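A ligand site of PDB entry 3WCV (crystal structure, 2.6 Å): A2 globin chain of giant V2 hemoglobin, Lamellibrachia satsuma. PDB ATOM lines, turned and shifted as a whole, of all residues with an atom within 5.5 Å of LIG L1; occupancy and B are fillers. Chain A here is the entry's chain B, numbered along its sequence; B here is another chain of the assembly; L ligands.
An oxygen (O1) of LG3 L3 is in hydrogen-bond range of the side-chain amide nitrogen (NE2) of Gln 94 of chain A (3.2 Å).
NE2 of Gln 98 of chain B sits at hydrogen-bond distance from O1 of LIG L1 (3.2 Å).
NH2 of Arg 49 is in salt-bridge range of O3 of LIG L1, 2.6 Å away.
A ring nitrogen (NE2) of His 63 is in hydrogen-bond range of an oxygen (O2) of LG2 L2 (2.9 Å).
An oxygen (O1) of LIG L1 sits at hydrogen-bond distance from a ring nitrogen (NE2) of His 94 of chain B (2.8 Å).
A ring nitrogen (NE2) of His 95 binds an iron atom (FE1) of LIG L1, at 2.1 Å.
The side-chain sulfur of Cys 74 is in hydrogen-bond range of the backbone carbonyl oxygen of Gly 70 (3.3 Å).
A ring nitrogen (ND1) of His 95 is in hydrogen-bond range of the backbone carbonyl oxygen (O) of Leu 91 (2.8 Å).
The backbone carbonyl oxygen (O) of Gln 94 of chain A lies within hydrogen-bond range of the guanidinium group (NE) of Arg 98 of chain A (3.0 Å).
The side-chain sulfur of Met 46 lies close to the side-chain amide oxygen of Gln 104, at 3.6 Å.
An iron atom (FE1) of LIG L1 is bound by an oxygen (O1) of LG2 L2, 1.8 Å away.
Met 46 touches LIG L1 (O to C31, 3.3 Å).
Phe 47 touches LIG L1 (CZ to C4, 3.5 Å).
CG1 of Val 50 touches O4 of LIG L1, at 3.5 Å.
His 63 touches LIG L1.
Arg 66 touches LIG L1 (O to C9, 3.4 Å).
O of Val 67 touches C17 of LIG L1, at 3.9 Å.
Gly 70 touches LIG L1 (C to C17, 3.9 Å).
Leu 71 touches LIG L1 (N to C17, 3.9 Å).
CD2 of Leu 91 touches C2 of LIG L1 (3.8 Å).
NE2 of Gln 94 of chain A touches C11 of LIG L1, at 3.6 Å.
Arg 98 of chain A touches LIG L1 (CZ to C32, 3.5 Å).
Val 100 touches LIG L1.
Gln 104 touches LIG L1.
CA of Tyr 105 touches C24 of LIG L1, at 3.6 Å.
Val 108 touches LIG L1.
CD1 of Ile 141 touches C18 of LIG L1 (3.8 Å).
Hydrophobic or aromatic side chains that line LIG L1: Met 46, Phe 47, Val 50, His 63, Leu 91, His 95, Val 100, Tyr 105, Val 108, Ile 141 and His 94 of chain B.
Of the 26 residues printed, 20 come within 4 Å of LIG L1.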
ATOM      1  N   TRP A  33      34.096  32.227 -27.232  1.00  0.00           N
ATOM      2  CA  TRP A  33      34.391  32.789 -25.921  1.00  0.00           C
ATOM      3  C   TRP A  33      35.210  34.075 -25.897  1.00  0.00           C
ATOM      4  O   TRP A  33      35.235  34.764 -24.887  1.00  0.00           O
ATOM      5  CB  TRP A  33      35.045  31.726 -25.040  1.00  0.00           C
ATOM      6  CG  TRP A  33      34.063  30.730 -24.565  1.00  0.00           C
ATOM      7  CD1 TRP A  33      33.757  29.533 -25.136  1.00  0.00           C
ATOM      8  CD2 TRP A  33      33.187  30.869 -23.447  1.00  0.00           C
ATOM      9  NE1 TRP A  33      32.737  28.921 -24.452  1.00  0.00           N
ATOM     10  CE2 TRP A  33      32.368  29.728 -23.409  1.00  0.00           C
ATOM     11  CE3 TRP A  33      33.022  31.862 -22.479  1.00  0.00           C
ATOM     12  CZ2 TRP A  33      31.394  29.535 -22.432  1.00  0.00           C
ATOM     13  CZ3 TRP A  33      32.044  31.678 -21.511  1.00  0.00           C
ATOM     14  CH2 TRP A  33      31.250  30.525 -21.493  1.00  0.00           C
ATOM     15  N   ALA A  43      31.803  38.764 -16.691  1.00  0.00           N
ATOM     16  CA  ALA A  43      31.446  37.347 -16.548  1.00  0.00           C
ATOM     17  C   ALA A  43      32.593  36.371 -16.291  1.00  0.00           C
ATOM     18  O   ALA A  43      32.361  35.268 -15.770  1.00  0.00           O
ATOM     19  CB  ALA A  43      30.659  36.895 -17.759  1.00  0.00           C
ATOM     20  N   MET A  46      33.179  34.178 -13.077  1.00  0.00           N
ATOM     21  CA  MET A  46      32.482  32.943 -12.745  1.00  0.00           C
ATOM     22  C   MET A  46      33.266  31.715 -13.183  1.00  0.00           C
ATOM     23  O   MET A  46      32.914  30.592 -12.833  1.00  0.00           O
ATOM     24  CB  MET A  46      31.119  32.919 -13.409  1.00  0.00           C
ATOM     25  CG  MET A  46      30.136  33.908 -12.850  1.00  0.00           C
ATOM     26  SD  MET A  46      28.667  33.952 -13.890  1.00  0.00           S
ATOM     27  CE  MET A  46      28.180  32.214 -13.803  1.00  0.00           C
ATOM     28  N   PHE A  47      34.327  31.934 -13.941  1.00  0.00           N
ATOM     29  CA  PHE A  47      35.124  30.847 -14.459  1.00  0.00           C
ATOM     30  C   PHE A  47      36.497  30.706 -13.808  1.00  0.00           C
ATOM     31  O   PHE A  47      37.439  30.191 -14.429  1.00  0.00           O
ATOM     32  CB  PHE A  47      35.288  31.033 -15.965  1.00  0.00           C
ATOM     33  CG  PHE A  47      33.995  31.016 -16.709  1.00  0.00           C
ATOM     34  CD1 PHE A  47      33.401  29.800 -17.051  1.00  0.00           C
ATOM     35  CD2 PHE A  47      33.369  32.202 -17.077  1.00  0.00           C
ATOM     36  CE1 PHE A  47      32.210  29.774 -17.749  1.00  0.00           C
ATOM     37  CE2 PHE A  47      32.166  32.184 -17.773  1.00  0.00           C
ATOM     38  CZ  PHE A  47      31.584  30.960 -18.116  1.00  0.00           C
ATOM     39  N   ARG A  49      37.717  28.622 -11.750  1.00  0.00           N
ATOM     40  CA  ARG A  49      38.243  27.255 -11.719  1.00  0.00           C
ATOM     41  C   ARG A  49      38.755  26.716 -13.061  1.00  0.00           C
ATOM     42  O   ARG A  49      39.509  25.741 -13.094  1.00  0.00           O
ATOM     43  CB  ARG A  49      37.181  26.295 -11.189  1.00  0.00           C
ATOM     44  CG  ARG A  49      37.752  24.929 -10.815  1.00  0.00           C
ATOM     45  CD  ARG A  49      36.642  23.976 -10.497  1.00  0.00           C
ATOM     46  NE  ARG A  49      35.877  23.635 -11.690  1.00  0.00           N
ATOM     47  CZ  ARG A  49      36.310  22.798 -12.619  1.00  0.00           C
ATOM     48  NH1 ARG A  49      37.488  22.210 -12.484  1.00  0.00           N
ATOM     49  NH2 ARG A  49      35.553  22.521 -13.679  1.00  0.00           N
ATOM     50  N   VAL A  50      38.345  27.347 -14.157  1.00  0.00           N
ATOM     51  CA  VAL A  50      38.772  26.895 -15.475  1.00  0.00           C
ATOM     52  C   VAL A  50      39.567  27.977 -16.188  1.00  0.00           C
ATOM     53  O   VAL A  50      39.503  28.105 -17.403  1.00  0.00           O
ATOM     54  CB  VAL A  50      37.548  26.468 -16.320  1.00  0.00           C
ATOM     55  CG1 VAL A  50      36.755  25.420 -15.564  1.00  0.00           C
ATOM     56  CG2 VAL A  50      36.673  27.664 -16.630  1.00  0.00           C
ATOM     57  N   HIS A  63      37.131  23.384 -20.981  1.00  0.00           N
ATOM     58  CA  HIS A  63      35.807  23.881 -20.601  1.00  0.00           C
ATOM     59  C   HIS A  63      35.052  24.225 -21.878  1.00  0.00           C
ATOM     60  O   HIS A  63      33.935  23.747 -22.095  1.00  0.00           O
ATOM     61  CB  HIS A  63      35.928  25.136 -19.713  1.00  0.00           C
ATOM     62  CG  HIS A  63      34.649  25.896 -19.581  1.00  0.00           C
ATOM     63  ND1 HIS A  63      33.582  25.446 -18.833  1.00  0.00           N
ATOM     64  CD2 HIS A  63      34.238  27.050 -20.160  1.00  0.00           C
ATOM     65  CE1 HIS A  63      32.570  26.289 -18.951  1.00  0.00           C
ATOM     66  NE2 HIS A  63      32.947  27.278 -19.750  1.00  0.00           N
ATOM     67  N   ARG A  66      33.636  21.316 -23.322  1.00  0.00           N
ATOM     68  CA  ARG A  66      32.433  20.852 -22.632  1.00  0.00           C
ATOM     69  C   ARG A  66      31.207  21.672 -22.983  1.00  0.00           C
ATOM     70  O   ARG A  66      30.106  21.124 -23.120  1.00  0.00           O
ATOM     71  CB  ARG A  66      32.648  20.858 -21.114  1.00  0.00           C
ATOM     72  CG  ARG A  66      33.622  19.803 -20.617  1.00  0.00           C
ATOM     73  CD  ARG A  66      33.594  19.694 -19.104  1.00  0.00           C
ATOM     74  NE  ARG A  66      34.097  20.909 -18.474  1.00  0.00           N
ATOM     75  CZ  ARG A  66      35.382  21.183 -18.294  1.00  0.00           C
ATOM     76  NH1 ARG A  66      35.742  22.330 -17.710  1.00  0.00           N
ATOM     77  NH2 ARG A  66      36.305  20.301 -18.665  1.00  0.00           N
ATOM     78  N   VAL A  67      31.374  22.980 -23.135  1.00  0.00           N
ATOM     79  CA  VAL A  67      30.235  23.826 -23.461  1.00  0.00           C
ATOM     80  C   VAL A  67      29.681  23.506 -24.841  1.00  0.00           C
ATOM     81  O   VAL A  67      28.475  23.310 -25.002  1.00  0.00           O
ATOM     82  CB  VAL A  67      30.597  25.324 -23.444  1.00  0.00           C
ATOM     83  CG1 VAL A  67      29.413  26.145 -23.942  1.00  0.00           C
ATOM     84  CG2 VAL A  67      30.974  25.759 -22.042  1.00  0.00           C
ATOM     85  N   GLY A  70      27.896  20.527 -25.052  1.00  0.00           N
ATOM     86  CA  GLY A  70      26.562  20.675 -24.501  1.00  0.00           C
ATOM     87  C   GLY A  70      25.583  21.222 -25.518  1.00  0.00           C
ATOM     88  O   GLY A  70      24.409  20.830 -25.556  1.00  0.00           O
ATOM     89  N   LEU A  71      26.046  22.165 -26.331  1.00  0.00           N
ATOM     90  CA  LEU A  71      25.204  22.759 -27.371  1.00  0.00           C
ATOM     91  C   LEU A  71      24.885  21.672 -28.403  1.00  0.00           C
ATOM     92  O   LEU A  71      23.749  21.555 -28.871  1.00  0.00           O
ATOM     93  CB  LEU A  71      25.930  23.910 -28.052  1.00  0.00           C
ATOM     94  CG  LEU A  71      25.649  25.333 -27.583  1.00  0.00           C
ATOM     95  CD1 LEU A  71      26.589  26.323 -28.284  1.00  0.00           C
ATOM     96  CD2 LEU A  71      24.197  25.663 -27.886  1.00  0.00           C
ATOM     97  N   CYS A  74      22.106  19.393 -27.403  1.00  0.00           N
ATOM     98  CA  CYS A  74      20.817  20.045 -27.538  1.00  0.00           C
ATOM     99  C   CYS A  74      20.422  20.180 -28.986  1.00  0.00           C
ATOM    100  O   CYS A  74      19.280  19.896 -29.320  1.00  0.00           O
ATOM    101  CB  CYS A  74      20.820  21.442 -26.898  1.00  0.00           C
ATOM    102  SG  CYS A  74      21.245  21.465 -25.160  1.00  0.00           S
ATOM    103  N   LEU A  91      21.520  20.255 -17.848  1.00  0.00           N
ATOM    104  CA  LEU A  91      22.334  21.447 -17.987  1.00  0.00           C
ATOM    105  C   LEU A  91      21.907  22.450 -16.926  1.00  0.00           C
ATOM    106  O   LEU A  91      22.749  23.118 -16.311  1.00  0.00           O
ATOM    107  CB  LEU A  91      22.168  22.058 -19.386  1.00  0.00           C
ATOM    108  CG  LEU A  91      22.919  21.349 -20.519  1.00  0.00           C
ATOM    109  CD1 LEU A  91      22.489  21.922 -21.871  1.00  0.00           C
ATOM    110  CD2 LEU A  91      24.417  21.502 -20.310  1.00  0.00           C
ATOM    111  N   GLN A  94      23.450  21.776 -13.724  1.00  0.00           N
ATOM    112  CA  GLN A  94      24.892  22.011 -13.710  1.00  0.00           C
ATOM    113  C   GLN A  94      25.195  23.498 -13.560  1.00  0.00           C
ATOM    114  O   GLN A  94      26.326  23.858 -13.239  1.00  0.00           O
ATOM    115  CB  GLN A  94      25.530  21.461 -15.005  1.00  0.00           C
ATOM    116  CG  GLN A  94      25.412  19.937 -15.166  1.00  0.00           C
ATOM    117  CD  GLN A  94      26.031  19.410 -16.462  1.00  0.00           C
ATOM    118  OE1 GLN A  94      25.658  19.838 -17.567  1.00  0.00           O
ATOM    119  NE2 GLN A  94      26.973  18.484 -16.339  1.00  0.00           N
ATOM    120  N   HIS A  95      24.188  24.339 -13.773  1.00  0.00           N
ATOM    121  CA  HIS A  95      24.326  25.787 -13.664  1.00  0.00           C
ATOM    122  C   HIS A  95      23.533  26.415 -12.514  1.00  0.00           C
ATOM    123  O   HIS A  95      23.666  27.599 -12.233  1.00  0.00           O
ATOM    124  CB  HIS A  95      23.866  26.472 -14.957  1.00  0.00           C
ATOM    125  CG  HIS A  95      24.742  26.200 -16.133  1.00  0.00           C
ATOM    126  ND1 HIS A  95      24.866  24.947 -16.698  1.00  0.00           N
ATOM    127  CD2 HIS A  95      25.541  27.017 -16.864  1.00  0.00           C
ATOM    128  CE1 HIS A  95      25.692  25.000 -17.721  1.00  0.00           C
ATOM    129  NE2 HIS A  95      26.124  26.242 -17.848  1.00  0.00           N
ATOM    130  N   ARG A  98      25.196  28.642  -9.668  1.00  0.00           N
ATOM    131  CA  ARG A  98      26.170  29.572 -10.205  1.00  0.00           C
ATOM    132  C   ARG A  98      25.634  30.965 -10.514  1.00  0.00           C
ATOM    133  O   ARG A  98      26.373  31.876 -10.864  1.00  0.00           O
ATOM    134  CB  ARG A  98      26.812  28.954 -11.456  1.00  0.00           C
ATOM    135  CG  ARG A  98      27.461  27.597 -11.173  1.00  0.00           C
ATOM    136  CD  ARG A  98      27.983  26.953 -12.437  1.00  0.00           C
ATOM    137  NE  ARG A  98      28.497  25.608 -12.206  1.00  0.00           N
ATOM    138  CZ  ARG A  98      29.596  25.324 -11.526  1.00  0.00           C
ATOM    139  NH1 ARG A  98      29.960  24.064 -11.373  1.00  0.00           N
ATOM    140  NH2 ARG A  98      30.322  26.299 -10.986  1.00  0.00           N
ATOM    141  N   VAL A 100      23.576  32.447 -13.031  1.00  0.00           N
ATOM    142  CA  VAL A 100      23.770  32.985 -14.364  1.00  0.00           C
ATOM    143  C   VAL A 100      22.545  33.826 -14.675  1.00  0.00           C
ATOM    144  O   VAL A 100      21.413  33.371 -14.473  1.00  0.00           O
ATOM    145  CB  VAL A 100      23.897  31.846 -15.413  1.00  0.00           C
ATOM    146  CG1 VAL A 100      24.078  32.440 -16.798  1.00  0.00           C
ATOM    147  CG2 VAL A 100      25.060  30.940 -15.052  1.00  0.00           C
ATOM    148  N   GLN A 104      23.322  37.084 -19.438  1.00  0.00           N
ATOM    149  CA  GLN A 104      24.593  36.459 -19.782  1.00  0.00           C
ATOM    150  C   GLN A 104      24.255  35.333 -20.763  1.00  0.00           C
ATOM    151  O   GLN A 104      25.013  35.066 -21.698  1.00  0.00           O
ATOM    152  CB  GLN A 104      25.273  35.897 -18.519  1.00  0.00           C
ATOM    153  CG  GLN A 104      25.722  36.955 -17.521  1.00  0.00           C
ATOM    154  CD  GLN A 104      26.412  36.352 -16.302  1.00  0.00           C
ATOM    155  OE1 GLN A 104      25.866  35.469 -15.636  1.00  0.00           O
ATOM    156  NE2 GLN A 104      27.607  36.843 -15.999  1.00  0.00           N
ATOM    157  N   TYR A 105      23.099  34.699 -20.565  1.00  0.00           N
ATOM    158  CA  TYR A 105      22.663  33.643 -21.473  1.00  0.00           C
ATOM    159  C   TYR A 105      22.480  34.226 -22.873  1.00  0.00           C
ATOM    160  O   TYR A 105      22.851  33.596 -23.864  1.00  0.00           O
ATOM    161  CB  TYR A 105      21.352  33.002 -21.001  1.00  0.00           C
ATOM    162  CG  TYR A 105      21.527  31.871 -20.007  1.00  0.00           C
ATOM    163  CD1 TYR A 105      22.129  30.677 -20.386  1.00  0.00           C
ATOM    164  CD2 TYR A 105      21.126  32.021 -18.678  1.00  0.00           C
ATOM    165  CE1 TYR A 105      22.330  29.642 -19.470  1.00  0.00           C
ATOM    166  CE2 TYR A 105      21.320  30.998 -17.748  1.00  0.00           C
ATOM    167  CZ  TYR A 105      21.922  29.808 -18.144  1.00  0.00           C
ATOM    168  OH  TYR A 105      22.133  28.802 -17.234  1.00  0.00           O
ATOM    169  N   VAL A 108      26.043  34.811 -24.596  1.00  0.00           N
ATOM    170  CA  VAL A 108      26.565  33.579 -25.138  1.00  0.00           C
ATOM    171  C   VAL A 108      25.807  33.213 -26.419  1.00  0.00           C
ATOM    172  O   VAL A 108      26.381  32.678 -27.368  1.00  0.00           O
ATOM    173  CB  VAL A 108      26.459  32.475 -24.089  1.00  0.00           C
ATOM    174  CG1 VAL A 108      26.757  31.120 -24.703  1.00  0.00           C
ATOM    175  CG2 VAL A 108      27.433  32.761 -22.965  1.00  0.00           C
ATOM    176  N   VAL A 112      27.661  32.566 -29.834  1.00  0.00           N
ATOM    177  CA  VAL A 112      27.491  31.326 -30.578  1.00  0.00           C
ATOM    178  C   VAL A 112      27.049  31.622 -32.015  1.00  0.00           C
ATOM    179  O   VAL A 112      27.552  31.016 -32.958  1.00  0.00           O
ATOM    180  CB  VAL A 112      26.449  30.410 -29.920  1.00  0.00           C
ATOM    181  CG1 VAL A 112      26.043  29.306 -30.886  1.00  0.00           C
ATOM    182  CG2 VAL A 112      27.024  29.802 -28.645  1.00  0.00           C
ATOM    183  N   ILE A 137      16.728  26.824 -26.188  1.00  0.00           N
ATOM    184  CA  ILE A 137      17.754  26.090 -25.454  1.00  0.00           C
ATOM    185  C   ILE A 137      18.159  26.717 -24.139  1.00  0.00           C
ATOM    186  O   ILE A 137      18.215  26.037 -23.118  1.00  0.00           O
ATOM    187  CB  ILE A 137      19.005  25.868 -26.337  1.00  0.00           C
ATOM    188  CG1 ILE A 137      18.626  24.938 -27.500  1.00  0.00           C
ATOM    189  CG2 ILE A 137      20.145  25.268 -25.513  1.00  0.00           C
ATOM    190  CD1 ILE A 137      19.723  24.729 -28.529  1.00  0.00           C
ATOM    191  N   THR A 138      18.447  28.015 -24.150  1.00  0.00           N
ATOM    192  CA  THR A 138      18.844  28.699 -22.928  1.00  0.00           C
ATOM    193  C   THR A 138      17.640  28.750 -22.006  1.00  0.00           C
ATOM    194  O   THR A 138      17.750  28.499 -20.806  1.00  0.00           O
ATOM    195  CB  THR A 138      19.301  30.141 -23.206  1.00  0.00           C
ATOM    196  OG1 THR A 138      18.270  30.855 -23.885  1.00  0.00           O
ATOM    197  CG2 THR A 138      20.565  30.126 -24.043  1.00  0.00           C
ATOM    198  N   ILE A 141      17.497  25.858 -20.021  1.00  0.00           N
ATOM    199  CA  ILE A 141      18.615  25.688 -19.103  1.00  0.00           C
ATOM    200  C   ILE A 141      18.393  26.551 -17.863  1.00  0.00           C
ATOM    201  O   ILE A 141      18.973  26.296 -16.805  1.00  0.00           O
ATOM    202  CB  ILE A 141      19.969  26.075 -19.749  1.00  0.00           C
ATOM    203  CG1 ILE A 141      20.223  25.209 -20.983  1.00  0.00           C
ATOM    204  CG2 ILE A 141      21.098  25.892 -18.744  1.00  0.00           C
ATOM    205  CD1 ILE A 141      21.507  25.521 -21.729  1.00  0.00           C
ATOM    206  N   HIS B  94      38.756  16.152 -15.744  1.00  0.00           N
ATOM    207  CA  HIS B  94      37.412  16.522 -15.409  1.00  0.00           C
ATOM    208  C   HIS B  94      36.506  15.285 -15.436  1.00  0.00           C
ATOM    209  O   HIS B  94      35.668  15.112 -14.557  1.00  0.00           O
ATOM    210  CB  HIS B  94      36.899  17.535 -16.399  1.00  0.00           C
ATOM    211  CG  HIS B  94      35.562  18.085 -16.055  1.00  0.00           C
ATOM    212  ND1 HIS B  94      35.397  19.206 -15.277  1.00  0.00           N
ATOM    213  CD2 HIS B  94      34.311  17.688 -16.409  1.00  0.00           C
ATOM    214  CE1 HIS B  94      34.109  19.487 -15.175  1.00  0.00           C
ATOM    215  NE2 HIS B  94      33.432  18.576 -15.853  1.00  0.00           N
ATOM    216  N   GLN B  98      34.442  13.153 -12.454  1.00  0.00           N
ATOM    217  CA  GLN B  98      33.008  12.908 -12.623  1.00  0.00           C
ATOM    218  C   GLN B  98      32.680  11.434 -12.362  1.00  0.00           C
ATOM    219  O   GLN B  98      31.522  11.089 -12.124  1.00  0.00           O
ATOM    220  CB  GLN B  98      32.544  13.321 -14.029  1.00  0.00           C
ATOM    221  CG  GLN B  98      32.441  14.841 -14.244  1.00  0.00           C
ATOM    222  CD  GLN B  98      31.871  15.199 -15.605  1.00  0.00           C
ATOM    223  OE1 GLN B  98      32.310  14.666 -16.627  1.00  0.00           O
ATOM    224  NE2 GLN B  98      30.917  16.114 -15.641  1.00  0.00           N
HETATM  225  C1  LIG L   1      29.740  24.858 -17.085  1.00  0.00           C
HETATM  226  C2  LIG L   1      27.078  24.203 -20.922  1.00  0.00           C
HETATM  227  C3  LIG L   1      25.843  28.868 -20.939  1.00  0.00           C
HETATM  228  C4  LIG L   1      28.577  29.503 -17.033  1.00  0.00           C
HETATM  229  C5  LIG L   1      29.132  24.258 -18.137  1.00  0.00           C
HETATM  230  C6  LIG L   1      29.273  22.888 -18.443  1.00  0.00           C
HETATM  231  C7  LIG L   1      28.522  22.691 -19.539  1.00  0.00           C
HETATM  232  C8  LIG L   1      27.892  23.951 -19.914  1.00  0.00           C
HETATM  233  C9  LIG L   1      28.323  21.366 -20.284  1.00  0.00           C
HETATM  234  C10 LIG L   1      30.105  21.856 -17.719  1.00  0.00           C
HETATM  235  C11 LIG L   1      29.382  21.216 -16.564  1.00  0.00           C
HETATM  236  C12 LIG L   1      30.212  20.167 -15.826  1.00  0.00           C
HETATM  237  O1  LIG L   1      30.723  19.211 -16.461  1.00  0.00           O
HETATM  238  O2  LIG L   1      30.363  20.311 -14.651  1.00  0.00           O
HETATM  239  C13 LIG L   1      26.474  25.412 -21.297  1.00  0.00           C
HETATM  240  C14 LIG L   1      25.580  25.566 -22.435  1.00  0.00           C
HETATM  241  C15 LIG L   1      25.215  26.950 -22.424  1.00  0.00           C
HETATM  242  C16 LIG L   1      25.911  27.517 -21.313  1.00  0.00           C
HETATM  243  C17 LIG L   1      25.135  24.502 -23.368  1.00  0.00           C
HETATM  244  C18 LIG L   1      24.314  27.520 -23.405  1.00  0.00           C
HETATM  245  C19 LIG L   1      24.682  28.366 -24.342  1.00  0.00           C
HETATM  246  C20 LIG L   1      26.502  29.438 -19.863  1.00  0.00           C
HETATM  247  C21 LIG L   1      26.389  30.862 -19.544  1.00  0.00           C
HETATM  248  C22 LIG L   1      27.179  31.097 -18.404  1.00  0.00           C
HETATM  249  C23 LIG L   1      27.750  29.729 -18.083  1.00  0.00           C
HETATM  250  C24 LIG L   1      25.561  31.895 -20.309  1.00  0.00           C
HETATM  251  C25 LIG L   1      27.389  32.262 -17.760  1.00  0.00           C
HETATM  252  C26 LIG L   1      28.034  33.361 -17.951  1.00  0.00           C
HETATM  253  C27 LIG L   1      29.140  28.276 -16.693  1.00  0.00           C
HETATM  254  C28 LIG L   1      30.054  28.067 -15.514  1.00  0.00           C
HETATM  255  C29 LIG L   1      30.365  26.737 -15.555  1.00  0.00           C
HETATM  256  C30 LIG L   1      29.669  26.167 -16.720  1.00  0.00           C
HETATM  257  C31 LIG L   1      30.480  29.148 -14.547  1.00  0.00           C
HETATM  258  C32 LIG L   1      31.250  25.976 -14.592  1.00  0.00           C
HETATM  259  C33 LIG L   1      32.674  25.900 -15.002  1.00  0.00           C
HETATM  260  C34 LIG L   1      33.447  25.122 -14.028  1.00  0.00           C
HETATM  261  O3  LIG L   1      33.370  23.866 -14.040  1.00  0.00           O
HETATM  262  O4  LIG L   1      34.153  25.709 -13.208  1.00  0.00           O
HETATM  263  N1  LIG L   1      28.291  24.928 -19.030  1.00  0.00           N
HETATM  264  N2  LIG L   1      26.690  26.553 -20.616  1.00  0.00           N
HETATM  265  N3  LIG L   1      27.334  28.803 -18.962  1.00  0.00           N
HETATM  266  N4  LIG L   1      28.943  27.121 -17.353  1.00  0.00           N
HETATM  267 FE1  LIG L   1      27.820  26.862 -18.982  1.00  0.00          FE
HETATM  268  O1  LG2 L   2      29.247  27.443 -19.903  1.00  0.00           O
HETATM  269  O2  LG2 L   2      30.173  28.268 -19.820  1.00  0.00           O
HETATM  270  C1  LG3 L   3      28.459   9.572 -15.922  1.00  0.00           C
HETATM  271  C2  LG3 L   3      31.211   9.376 -19.757  1.00  0.00           C
HETATM  272  C3  LG3 L   3      32.541   4.861 -18.642  1.00  0.00           C
HETATM  273  C4  LG3 L   3      29.776   5.124 -14.715  1.00  0.00           C
HETATM  274  C5  LG3 L   3      29.087   9.932 -17.063  1.00  0.00           C
HETATM  275  C6  LG3 L   3      28.907  11.188 -17.675  1.00  0.00           C
HETATM  276  C7  LG3 L   3      29.703  11.144 -18.773  1.00  0.00           C
HETATM  277  C8  LG3 L   3      30.367   9.840 -18.833  1.00  0.00           C
HETATM  278  C9  LG3 L   3      29.894  12.250 -19.821  1.00  0.00           C
HETATM  279  C10 LG3 L   3      28.012  12.344 -17.208  1.00  0.00           C
HETATM  280  C11 LG3 L   3      28.726  13.387 -16.382  1.00  0.00           C
HETATM  281  C12 LG3 L   3      27.849  14.566 -15.897  1.00  0.00           C
HETATM  282  O1  LG3 L   3      27.278  15.319 -16.744  1.00  0.00           O
HETATM  283  O2  LG3 L   3      27.731  14.740 -14.719  1.00  0.00           O
HETATM  284  C13 LG3 L   3      31.841   8.112 -19.826  1.00  0.00           C
HETATM  285  C14 LG3 L   3      32.741   7.701 -20.903  1.00  0.00           C
HETATM  286  C15 LG3 L   3      33.128   6.347 -20.564  1.00  0.00           C
HETATM  287  C16 LG3 L   3      32.451   6.064 -19.329  1.00  0.00           C
HETATM  288  C17 LG3 L   3      33.143   8.504 -22.080  1.00  0.00           C
HETATM  289  C18 LG3 L   3      34.024   5.535 -21.369  1.00  0.00           C
HETATM  290  C19 LG3 L   3      35.340   5.586 -21.339  1.00  0.00           C
HETATM  291  C20 LG3 L   3      31.895   4.558 -17.459  1.00  0.00           C
HETATM  292  C21 LG3 L   3      32.055   3.245 -16.783  1.00  0.00           C
HETATM  293  C22 LG3 L   3      31.259   3.288 -15.614  1.00  0.00           C
HETATM  294  C23 LG3 L   3      30.641   4.672 -15.666  1.00  0.00           C
HETATM  295  C24 LG3 L   3      32.933   2.079 -17.264  1.00  0.00           C
HETATM  296  C25 LG3 L   3      31.096   2.313 -14.672  1.00  0.00           C
HETATM  297  C26 LG3 L   3      30.810   1.055 -14.582  1.00  0.00           C
HETATM  298  C27 LG3 L   3      29.157   6.378 -14.701  1.00  0.00           C
HETATM  299  C28 LG3 L   3      28.177   6.823 -13.624  1.00  0.00           C
HETATM  300  C29 LG3 L   3      27.817   8.084 -14.012  1.00  0.00           C
HETATM  301  C30 LG3 L   3      28.561   8.392 -15.246  1.00  0.00           C
HETATM  302  C31 LG3 L   3      27.741   5.992 -12.442  1.00  0.00           C
HETATM  303  C32 LG3 L   3      26.848   9.029 -13.327  1.00  0.00           C
HETATM  304  C33 LG3 L   3      25.509   8.919 -14.033  1.00  0.00           C
HETATM  305  C34 LG3 L   3      24.453   9.790 -13.513  1.00  0.00           C
HETATM  306  O3  LG3 L   3      23.712   9.388 -12.578  1.00  0.00           O
HETATM  307  O4  LG3 L   3      24.293  10.913 -14.018  1.00  0.00           O
HETATM  308  N1  LG3 L   3      29.981   9.093 -17.750  1.00  0.00           N
HETATM  309  N2  LG3 L   3      31.651   7.162 -18.891  1.00  0.00           N
HETATM  310  N3  LG3 L   3      31.041   5.374 -16.747  1.00  0.00           N
HETATM  311  N4  LG3 L   3      29.340   7.340 -15.621  1.00  0.00           N
HETATM  312 FE1  LG3 L   3      30.518   7.244 -17.246  1.00  0.00          FE
